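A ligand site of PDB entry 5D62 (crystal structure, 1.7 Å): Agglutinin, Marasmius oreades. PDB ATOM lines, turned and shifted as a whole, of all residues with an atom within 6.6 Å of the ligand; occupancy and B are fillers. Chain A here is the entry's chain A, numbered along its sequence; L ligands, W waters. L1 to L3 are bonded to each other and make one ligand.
Water W2 lies within hydrogen-bond range of O2 of LG3 L3 (2.7 Å), OG1 of Thr 41 (2.9 Å), O of Ile 42 (3.1 Å) and OD1 of Asn 43 (3.3 Å).
Water W1 lies within hydrogen-bond range of O4 of LG2 L2 (2.8 Å), N of His 45 (2.8 Å) and N of Trp 44 (3.2 Å).
Water W6 bridges OD1 of Asp 23 and O5 of LG2 L2.
Water W5 lies within hydrogen-bond range of O1 of LG3 L3, N of Trp 44 and O of Ile 42.
Water W3 bridges the side-chain carboxylate (OD2) of Asp 131 (3.1 Å) and an oxygen (O5) of LG3 L3 (3.1 Å).
The side-chain amide oxygen (OE1) of Gln 46 lies within hydrogen-bond range of a ring nitrogen (NE2) of His 9, at 2.9 Å.
ND2 of Asn 43 lies within hydrogen-bond range of O of Thr 38 (3.0 Å).
ND2 of Asn 43 is in hydrogen-bond range of OG1 of Thr 41 (3.3 Å).
The side-chain carboxylate (OD2) of Asp 131 is in hydrogen-bond range of the side-chain amide nitrogen (NE2) of Gln 36, 2.7 Å away.
OD2 of Asp 20 lies within hydrogen-bond range of NE2 of Gln 46, 2.9 Å away.
O of His 45 is in hydrogen-bond range of N of Leu 21 (3.1 Å).
A ring nitrogen (ND1) of His 45 lies within hydrogen-bond range of the backbone NH (N) of Gly 24, 3.5 Å away.
N of Asp 20 sits at hydrogen-bond distance from O of Val 33.
CA of Lys 22 touches O6 of LG2 L2, at 3.6 Å.
Phe 37 touches the ligand.
CB of Trp 44 touches C6 of LIG L1, 3.8 Å away.
NE2 of Gln 46 touches C1 of LG3 L3, at 3.8 Å.
Within 4 Å of the ligand: Asp 20, Leu 21, Lys 22, Asp 23, Trp 35, Gln 36, Phe 37, Thr 38, Asn 43, Trp 44, His 45 and Gln 46.
The nearest printed residue that does not touch the ligand is Gly 24 (4.3 Å).
The backbone carbonyl oxygen (O) of Gln 36 is in hydrogen-bond range of an oxygen (O3) of LG3 L3 (3.3 Å).
OD1 of Asp 20 is in hydrogen-bond range of O6 of LG2 L2 (2.5 Å).
The side-chain hydroxyl (OG1) of Thr 38 lies within hydrogen-bond range of an oxygen (O2) of LG3 L3.
An oxygen (O6) of LG2 L2 is in hydrogen-bond range of the backbone NH (N) of Asp 23, at 2.9 Å.
OD1 of Asn 43 lies within hydrogen-bond range of O1 of LG3 L3.
O2 of LG3 L3 lies within hydrogen-bond range of N of Thr 38, 3.3 Å away.
The indole nitrogen (NE1) of Trp 35 lies within hydrogen-bond range of an oxygen (O5) of LG3 L3 (3.0 Å).
A ring nitrogen (ND1) of His 45 is in hydrogen-bond range of an oxygen (O6) of LG2 L2, 3.0 Å away.
The backbone carbonyl oxygen (O) of Leu 21 lies within hydrogen-bond range of an oxygen (O6) of LG2 L2.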
ATOM      1  N   HIS A   9     -13.893 -27.974  13.731  1.00  0.00           N
ATOM      2  CA  HIS A   9     -13.932 -28.903  14.870  1.00  0.00           C
ATOM      3  C   HIS A   9     -14.055 -30.264  14.160  1.00  0.00           C
ATOM      4  O   HIS A   9     -14.995 -30.499  13.391  1.00  0.00           O
ATOM      5  CB  HIS A   9     -15.141 -28.567  15.699  1.00  0.00           C
ATOM      6  CG  HIS A   9     -15.259 -29.394  16.931  1.00  0.00           C
ATOM      7  ND1 HIS A   9     -16.131 -30.462  17.053  1.00  0.00           N
ATOM      8  CD2 HIS A   9     -14.524 -29.370  18.071  1.00  0.00           C
ATOM      9  CE1 HIS A   9     -15.983 -30.990  18.244  1.00  0.00           C
ATOM     10  NE2 HIS A   9     -14.999 -30.369  18.878  1.00  0.00           N
ATOM     11  N   ASP A  20      -8.093 -33.546  19.405  1.00  0.00           N
ATOM     12  CA  ASP A  20      -7.832 -32.696  20.554  1.00  0.00           C
ATOM     13  C   ASP A  20      -6.256 -32.634  20.748  1.00  0.00           C
ATOM     14  O   ASP A  20      -5.586 -33.637  20.846  1.00  0.00           O
ATOM     15  CB  ASP A  20      -8.499 -33.296  21.766  1.00  0.00           C
ATOM     16  CG  ASP A  20      -8.396 -32.435  23.075  1.00  0.00           C
ATOM     17  OD1 ASP A  20      -7.238 -32.241  23.605  1.00  0.00           O
ATOM     18  OD2 ASP A  20      -9.444 -31.982  23.651  1.00  0.00           O
ATOM     19  N   LEU A  21      -5.723 -31.464  20.875  1.00  0.00           N
ATOM     20  CA  LEU A  21      -4.276 -31.321  21.157  1.00  0.00           C
ATOM     21  C   LEU A  21      -4.206 -31.314  22.681  1.00  0.00           C
ATOM     22  O   LEU A  21      -4.754 -30.359  23.345  1.00  0.00           O
ATOM     23  CB  LEU A  21      -3.774 -29.982  20.624  1.00  0.00           C
ATOM     24  CG  LEU A  21      -2.327 -29.663  20.961  1.00  0.00           C
ATOM     25  CD1 LEU A  21      -1.361 -30.677  20.380  1.00  0.00           C
ATOM     26  CD2 LEU A  21      -1.901 -28.264  20.465  1.00  0.00           C
ATOM     27  N   LYS A  22      -3.576 -32.308  23.246  1.00  0.00           N
ATOM     28  CA  LYS A  22      -3.671 -32.560  24.711  1.00  0.00           C
ATOM     29  C   LYS A  22      -3.213 -31.362  25.537  1.00  0.00           C
ATOM     30  O   LYS A  22      -2.104 -30.835  25.378  1.00  0.00           O
ATOM     31  CB  LYS A  22      -2.962 -33.891  25.113  1.00  0.00           C
ATOM     32  CG  LYS A  22      -3.626 -34.512  26.263  1.00  0.00           C
ATOM     33  CD  LYS A  22      -2.848 -35.786  26.682  1.00  0.00           C
ATOM     34  CE  LYS A  22      -3.608 -36.349  27.899  1.00  0.00           C
ATOM     35  NZ  LYS A  22      -3.037 -37.761  28.139  1.00  0.00           N
ATOM     36  N   ASP A  23      -4.098 -30.955  26.456  1.00  0.00           N
ATOM     37  CA  ASP A  23      -3.948 -29.753  27.282  1.00  0.00           C
ATOM     38  C   ASP A  23      -3.690 -28.461  26.564  1.00  0.00           C
ATOM     39  O   ASP A  23      -3.234 -27.504  27.174  1.00  0.00           O
ATOM     40  CB  ASP A  23      -2.826 -29.987  28.314  1.00  0.00           C
ATOM     41  CG  ASP A  23      -3.041 -29.223  29.625  1.00  0.00           C
ATOM     42  OD1 ASP A  23      -4.159 -29.041  30.109  1.00  0.00           O
ATOM     43  OD2 ASP A  23      -2.032 -28.773  30.206  1.00  0.00           O
ATOM     44  N   GLY A  24      -3.905 -28.429  25.268  1.00  0.00           N
ATOM     45  CA  GLY A  24      -3.667 -27.278  24.490  1.00  0.00           C
ATOM     46  C   GLY A  24      -2.196 -26.911  24.459  1.00  0.00           C
ATOM     47  O   GLY A  24      -1.880 -25.784  24.099  1.00  0.00           O
ATOM     48  N   VAL A  33      -5.097 -36.398  20.318  1.00  0.00           N
ATOM     49  CA  VAL A  33      -5.816 -37.500  20.902  1.00  0.00           C
ATOM     50  C   VAL A  33      -7.278 -37.331  20.615  1.00  0.00           C
ATOM     51  O   VAL A  33      -7.772 -36.188  20.364  1.00  0.00           O
ATOM     52  CB  VAL A  33      -5.635 -37.638  22.488  1.00  0.00           C
ATOM     53  CG1 VAL A  33      -4.209 -38.061  22.850  1.00  0.00           C
ATOM     54  CG2 VAL A  33      -6.019 -36.384  23.223  1.00  0.00           C
ATOM     55  N   TRP A  35     -11.009 -37.006  22.141  1.00  0.00           N
ATOM     56  CA  TRP A  35     -11.598 -36.429  23.378  1.00  0.00           C
ATOM     57  C   TRP A  35     -13.046 -36.034  23.141  1.00  0.00           C
ATOM     58  O   TRP A  35     -13.403 -35.475  22.115  1.00  0.00           O
ATOM     59  CB  TRP A  35     -10.793 -35.228  23.875  1.00  0.00           C
ATOM     60  CG  TRP A  35     -10.833 -34.987  25.349  1.00  0.00           C
ATOM     61  CD1 TRP A  35     -11.849 -34.462  26.075  1.00  0.00           C
ATOM     62  CD2 TRP A  35      -9.826 -35.347  26.277  1.00  0.00           C
ATOM     63  NE1 TRP A  35     -11.535 -34.440  27.431  1.00  0.00           N
ATOM     64  CE2 TRP A  35     -10.304 -34.989  27.590  1.00  0.00           C
ATOM     65  CE3 TRP A  35      -8.559 -35.945  26.140  1.00  0.00           C
ATOM     66  CZ2 TRP A  35      -9.559 -35.221  28.763  1.00  0.00           C
ATOM     67  CZ3 TRP A  35      -7.826 -36.195  27.314  1.00  0.00           C
ATOM     68  CH2 TRP A  35      -8.337 -35.820  28.622  1.00  0.00           C
ATOM     69  N   GLN A  36     -13.896 -36.205  24.147  1.00  0.00           N
ATOM     70  CA  GLN A  36     -15.267 -35.758  24.069  1.00  0.00           C
ATOM     71  C   GLN A  36     -15.396 -34.258  24.050  1.00  0.00           C
ATOM     72  O   GLN A  36     -14.482 -33.547  24.413  1.00  0.00           O
ATOM     73  CB  GLN A  36     -16.121 -36.353  25.207  1.00  0.00           C
ATOM     74  CG  GLN A  36     -15.835 -35.792  26.574  1.00  0.00           C
ATOM     75  CD  GLN A  36     -16.662 -36.467  27.670  1.00  0.00           C
ATOM     76  OE1 GLN A  36     -17.858 -36.307  27.701  1.00  0.00           O
ATOM     77  NE2 GLN A  36     -16.035 -37.233  28.538  1.00  0.00           N
ATOM     78  N   PHE A  37     -16.575 -33.739  23.650  1.00  0.00           N
ATOM     79  CA  PHE A  37     -16.765 -32.326  23.423  1.00  0.00           C
ATOM     80  C   PHE A  37     -18.161 -31.915  23.828  1.00  0.00           C
ATOM     81  O   PHE A  37     -19.021 -32.823  24.086  1.00  0.00           O
ATOM     82  CB  PHE A  37     -16.474 -32.009  21.913  1.00  0.00           C
ATOM     83  CG  PHE A  37     -17.441 -32.661  20.962  1.00  0.00           C
ATOM     84  CD1 PHE A  37     -17.151 -33.879  20.422  1.00  0.00           C
ATOM     85  CD2 PHE A  37     -18.556 -31.997  20.548  1.00  0.00           C
ATOM     86  CE1 PHE A  37     -18.010 -34.484  19.504  1.00  0.00           C
ATOM     87  CE2 PHE A  37     -19.492 -32.639  19.687  1.00  0.00           C
ATOM     88  CZ  PHE A  37     -19.165 -33.870  19.184  1.00  0.00           C
ATOM     89  N   THR A  38     -18.357 -30.608  23.924  1.00  0.00           N
ATOM     90  CA  THR A  38     -19.685 -30.056  24.278  1.00  0.00           C
ATOM     91  C   THR A  38     -20.114 -29.207  23.076  1.00  0.00           C
ATOM     92  O   THR A  38     -19.410 -28.274  22.713  1.00  0.00           O
ATOM     93  CB  THR A  38     -19.605 -29.222  25.590  1.00  0.00           C
ATOM     94  OG1 THR A  38     -18.999 -30.053  26.619  1.00  0.00           O
ATOM     95  CG2 THR A  38     -20.960 -28.736  25.995  1.00  0.00           C
ATOM     96  N   PRO A  39     -21.246 -29.522  22.437  1.00  0.00           N
ATOM     97  CA  PRO A  39     -21.743 -28.662  21.301  1.00  0.00           C
ATOM     98  C   PRO A  39     -22.121 -27.275  21.731  1.00  0.00           C
ATOM     99  O   PRO A  39     -22.390 -27.065  22.905  1.00  0.00           O
ATOM    100  CB  PRO A  39     -22.976 -29.400  20.779  1.00  0.00           C
ATOM    101  CG  PRO A  39     -23.171 -30.569  21.679  1.00  0.00           C
ATOM    102  CD  PRO A  39     -22.204 -30.568  22.826  1.00  0.00           C
ATOM    103  N   THR A  41     -20.307 -24.676  22.330  1.00  0.00           N
ATOM    104  CA  THR A  41     -19.347 -24.066  23.228  1.00  0.00           C
ATOM    105  C   THR A  41     -18.078 -23.842  22.378  1.00  0.00           C
ATOM    106  O   THR A  41     -17.949 -24.445  21.300  1.00  0.00           O
ATOM    107  CB  THR A  41     -18.870 -24.965  24.374  1.00  0.00           C
ATOM    108  OG1 THR A  41     -18.152 -26.100  23.860  1.00  0.00           O
ATOM    109  CG2 THR A  41     -20.060 -25.427  25.210  1.00  0.00           C
ATOM    110  N   ILE A  42     -17.162 -23.045  22.895  1.00  0.00           N
ATOM    111  CA  ILE A  42     -15.770 -23.051  22.414  1.00  0.00           C
ATOM    112  C   ILE A  42     -15.090 -24.287  23.020  1.00  0.00           C
ATOM    113  O   ILE A  42     -14.903 -24.351  24.287  1.00  0.00           O
ATOM    114  CB  ILE A  42     -15.019 -21.769  22.799  1.00  0.00           C
ATOM    115  CG1 ILE A  42     -15.688 -20.539  22.098  1.00  0.00           C
ATOM    116  CG2 ILE A  42     -13.531 -21.945  22.492  1.00  0.00           C
ATOM    117  CD1 ILE A  42     -15.704 -20.527  20.588  1.00  0.00           C
ATOM    118  N   ASN A  43     -14.687 -25.245  22.161  1.00  0.00           N
ATOM    119  CA  ASN A  43     -13.847 -26.402  22.617  1.00  0.00           C
ATOM    120  C   ASN A  43     -12.421 -26.054  22.444  1.00  0.00           C
ATOM    121  O   ASN A  43     -11.870 -26.135  21.303  1.00  0.00           O
ATOM    122  CB  ASN A  43     -14.263 -27.680  21.853  1.00  0.00           C
ATOM    123  CG  ASN A  43     -15.673 -28.121  22.253  1.00  0.00           C
ATOM    124  OD1 ASN A  43     -15.846 -28.768  23.273  1.00  0.00           O
ATOM    125  ND2 ASN A  43     -16.702 -27.822  21.409  1.00  0.00           N
ATOM    126  N   TRP A  44     -11.849 -25.542  23.553  1.00  0.00           N
ATOM    127  CA  TRP A  44     -10.635 -24.747  23.516  1.00  0.00           C
ATOM    128  C   TRP A  44      -9.448 -25.464  22.892  1.00  0.00           C
ATOM    129  O   TRP A  44      -8.570 -24.813  22.250  1.00  0.00           O
ATOM    130  CB  TRP A  44     -10.225 -24.300  24.936  1.00  0.00           C
ATOM    131  CG  TRP A  44     -11.041 -23.119  25.348  1.00  0.00           C
ATOM    132  CD1 TRP A  44     -12.197 -23.136  26.134  1.00  0.00           C
ATOM    133  CD2 TRP A  44     -10.771 -21.727  24.996  1.00  0.00           C
ATOM    134  NE1 TRP A  44     -12.678 -21.819  26.233  1.00  0.00           N
ATOM    135  CE2 TRP A  44     -11.855 -20.961  25.521  1.00  0.00           C
ATOM    136  CE3 TRP A  44      -9.770 -21.097  24.217  1.00  0.00           C
ATOM    137  CZ2 TRP A  44     -11.925 -19.576  25.392  1.00  0.00           C
ATOM    138  CZ3 TRP A  44      -9.854 -19.743  24.042  1.00  0.00           C
ATOM    139  CH2 TRP A  44     -10.930 -18.972  24.654  1.00  0.00           C
ATOM    140  N   HIS A  45      -9.357 -26.779  23.074  1.00  0.00           N
ATOM    141  CA  HIS A  45      -8.181 -27.498  22.476  1.00  0.00           C
ATOM    142  C   HIS A  45      -8.435 -28.213  21.190  1.00  0.00           C
ATOM    143  O   HIS A  45      -7.585 -28.960  20.682  1.00  0.00           O
ATOM    144  CB  HIS A  45      -7.581 -28.433  23.515  1.00  0.00           C
ATOM    145  CG  HIS A  45      -7.315 -27.768  24.839  1.00  0.00           C
ATOM    146  ND1 HIS A  45      -7.300 -28.477  26.020  1.00  0.00           N
ATOM    147  CD2 HIS A  45      -6.918 -26.520  25.134  1.00  0.00           C
ATOM    148  CE1 HIS A  45      -6.966 -27.646  27.020  1.00  0.00           C
ATOM    149  NE2 HIS A  45      -6.695 -26.474  26.502  1.00  0.00           N
ATOM    150  N   GLN A  46      -9.624 -28.001  20.550  1.00  0.00           N
ATOM    151  CA  GLN A  46     -10.169 -28.848  19.503  1.00  0.00           C
ATOM    152  C   GLN A  46     -10.477 -28.069  18.220  1.00  0.00           C
ATOM    153  O   GLN A  46     -11.275 -28.549  17.407  1.00  0.00           O
ATOM    154  CB  GLN A  46     -11.438 -29.547  20.001  1.00  0.00           C
ATOM    155  CG  GLN A  46     -11.137 -30.436  21.270  1.00  0.00           C
ATOM    156  CD  GLN A  46     -12.382 -31.123  21.794  1.00  0.00           C
ATOM    157  OE1 GLN A  46     -13.511 -30.893  21.278  1.00  0.00           O
ATOM    158  NE2 GLN A  46     -12.218 -32.000  22.712  1.00  0.00           N
ATOM    159  N   PHE A  66      -5.716 -22.597  19.443  1.00  0.00           N
ATOM    160  CA  PHE A  66      -5.205 -22.262  20.747  1.00  0.00           C
ATOM    161  C   PHE A  66      -3.674 -22.303  20.868  1.00  0.00           C
ATOM    162  O   PHE A  66      -3.099 -21.292  21.340  1.00  0.00           O
ATOM    163  CB  PHE A  66      -5.788 -23.192  21.807  1.00  0.00           C
ATOM    164  CG  PHE A  66      -5.385 -22.855  23.214  1.00  0.00           C
ATOM    165  CD1 PHE A  66      -5.976 -21.718  23.886  1.00  0.00           C
ATOM    166  CD2 PHE A  66      -4.454 -23.586  23.915  1.00  0.00           C
ATOM    167  CE1 PHE A  66      -5.630 -21.391  25.170  1.00  0.00           C
ATOM    168  CE2 PHE A  66      -4.142 -23.276  25.276  1.00  0.00           C
ATOM    169  CZ  PHE A  66      -4.712 -22.184  25.883  1.00  0.00           C
ATOM    170  N   ASP A 131     -11.478 -40.648  26.546  1.00  0.00           N
ATOM    171  CA  ASP A 131     -10.827 -39.332  26.536  1.00  0.00           C
ATOM    172  C   ASP A 131      -9.293 -39.588  26.591  1.00  0.00           C
ATOM    173  O   ASP A 131      -8.747 -40.269  27.527  1.00  0.00           O
ATOM    174  CB  ASP A 131     -11.286 -38.451  27.724  1.00  0.00           C
ATOM    175  CG  ASP A 131     -12.704 -37.959  27.555  1.00  0.00           C
ATOM    176  OD1 ASP A 131     -13.128 -37.979  26.369  1.00  0.00           O
ATOM    177  OD2 ASP A 131     -13.320 -37.579  28.585  1.00  0.00           O
HETATM  178  C1  LIG L   1     -12.061 -27.942  29.228  1.00  0.00           C
HETATM  179  C2  LIG L   1     -12.771 -27.658  30.556  1.00  0.00           C
HETATM  180  C3  LIG L   1     -11.807 -26.876  31.472  1.00  0.00           C
HETATM  181  C4  LIG L   1     -11.182 -25.616  30.789  1.00  0.00           C
HETATM  182  C5  LIG L   1     -10.424 -26.146  29.525  1.00  0.00           C
HETATM  183  C6  LIG L   1      -9.810 -25.012  28.681  1.00  0.00           C
HETATM  184  O1  LIG L   1     -13.213 -28.920  31.059  1.00  0.00           O
HETATM  185  O2  LIG L   1     -12.600 -26.505  32.623  1.00  0.00           O
HETATM  186  O3  LIG L   1     -12.246 -24.658  30.470  1.00  0.00           O
HETATM  187  O4  LIG L   1     -11.380 -26.818  28.676  1.00  0.00           O
HETATM  188  C1  LG2 L   2      -8.954 -29.905  29.219  1.00  0.00           C
HETATM  189  C2  LG2 L   2     -10.202 -29.423  28.436  1.00  0.00           C
HETATM  190  C3  LG2 L   2     -10.898 -30.542  27.700  1.00  0.00           C
HETATM  191  C4  LG2 L   2      -9.949 -31.310  26.786  1.00  0.00           C
HETATM  192  C5  LG2 L   2      -8.640 -31.627  27.616  1.00  0.00           C
HETATM  193  C6  LG2 L   2      -7.586 -32.328  26.796  1.00  0.00           C
HETATM  194  O1  LG2 L   2      -8.281 -28.722  29.601  1.00  0.00           O
HETATM  195  O2  LG2 L   2     -11.069 -28.967  29.528  1.00  0.00           O
HETATM  196  O3  LG2 L   2     -12.046 -29.998  27.001  1.00  0.00           O
HETATM  197  O4  LG2 L   2      -9.626 -30.433  25.702  1.00  0.00           O
HETATM  198  O5  LG2 L   2      -8.045 -30.454  28.265  1.00  0.00           O
HETATM  199  O6  LG2 L   2      -6.853 -31.466  25.911  1.00  0.00           O
HETATM  200  C1  LG3 L   3     -12.848 -31.062  26.357  1.00  0.00           C
HETATM  201  C2  LG3 L   3     -14.065 -30.282  25.792  1.00  0.00           C
HETATM  202  C3  LG3 L   3     -15.127 -29.928  26.842  1.00  0.00           C
HETATM  203  C4  LG3 L   3     -15.484 -31.138  27.735  1.00  0.00           C
HETATM  204  C5  LG3 L   3     -14.128 -31.606  28.318  1.00  0.00           C
HETATM  205  C6  LG3 L   3     -14.214 -32.771  29.261  1.00  0.00           C
HETATM  206  O1  LG3 L   3     -13.730 -29.099  25.025  1.00  0.00           O
HETATM  207  O2  LG3 L   3     -16.330 -29.432  26.178  1.00  0.00           O
HETATM  208  O3  LG3 L   3     -16.077 -32.179  26.917  1.00  0.00           O
HETATM  209  O4  LG3 L   3     -13.321 -32.086  27.246  1.00  0.00           O
HETATM  210  O5  LG3 L   3     -12.924 -33.264  29.754  1.00  0.00           O
HETATM  211  O   HOH W   1     -11.103 -28.548  24.317  1.00  0.00           O
HETATM  212  O   HOH W   2     -16.150 -26.766  25.824  1.00  0.00           O
HETATM  213  O   HOH W   3     -12.244 -35.994  30.961  1.00  0.00           O
HETATM  214  O   HOH W   4     -11.850 -31.326  31.514  1.00  0.00           O
HETATM  215  O   HOH W   5     -13.304 -26.375  26.065  1.00  0.00           O
HETATM  216  O   HOH W   6      -5.854 -31.182  29.908  1.00  0.00           O
HETATM  217  O   HOH W   7     -14.157 -25.058  28.560  1.00  0.00           O
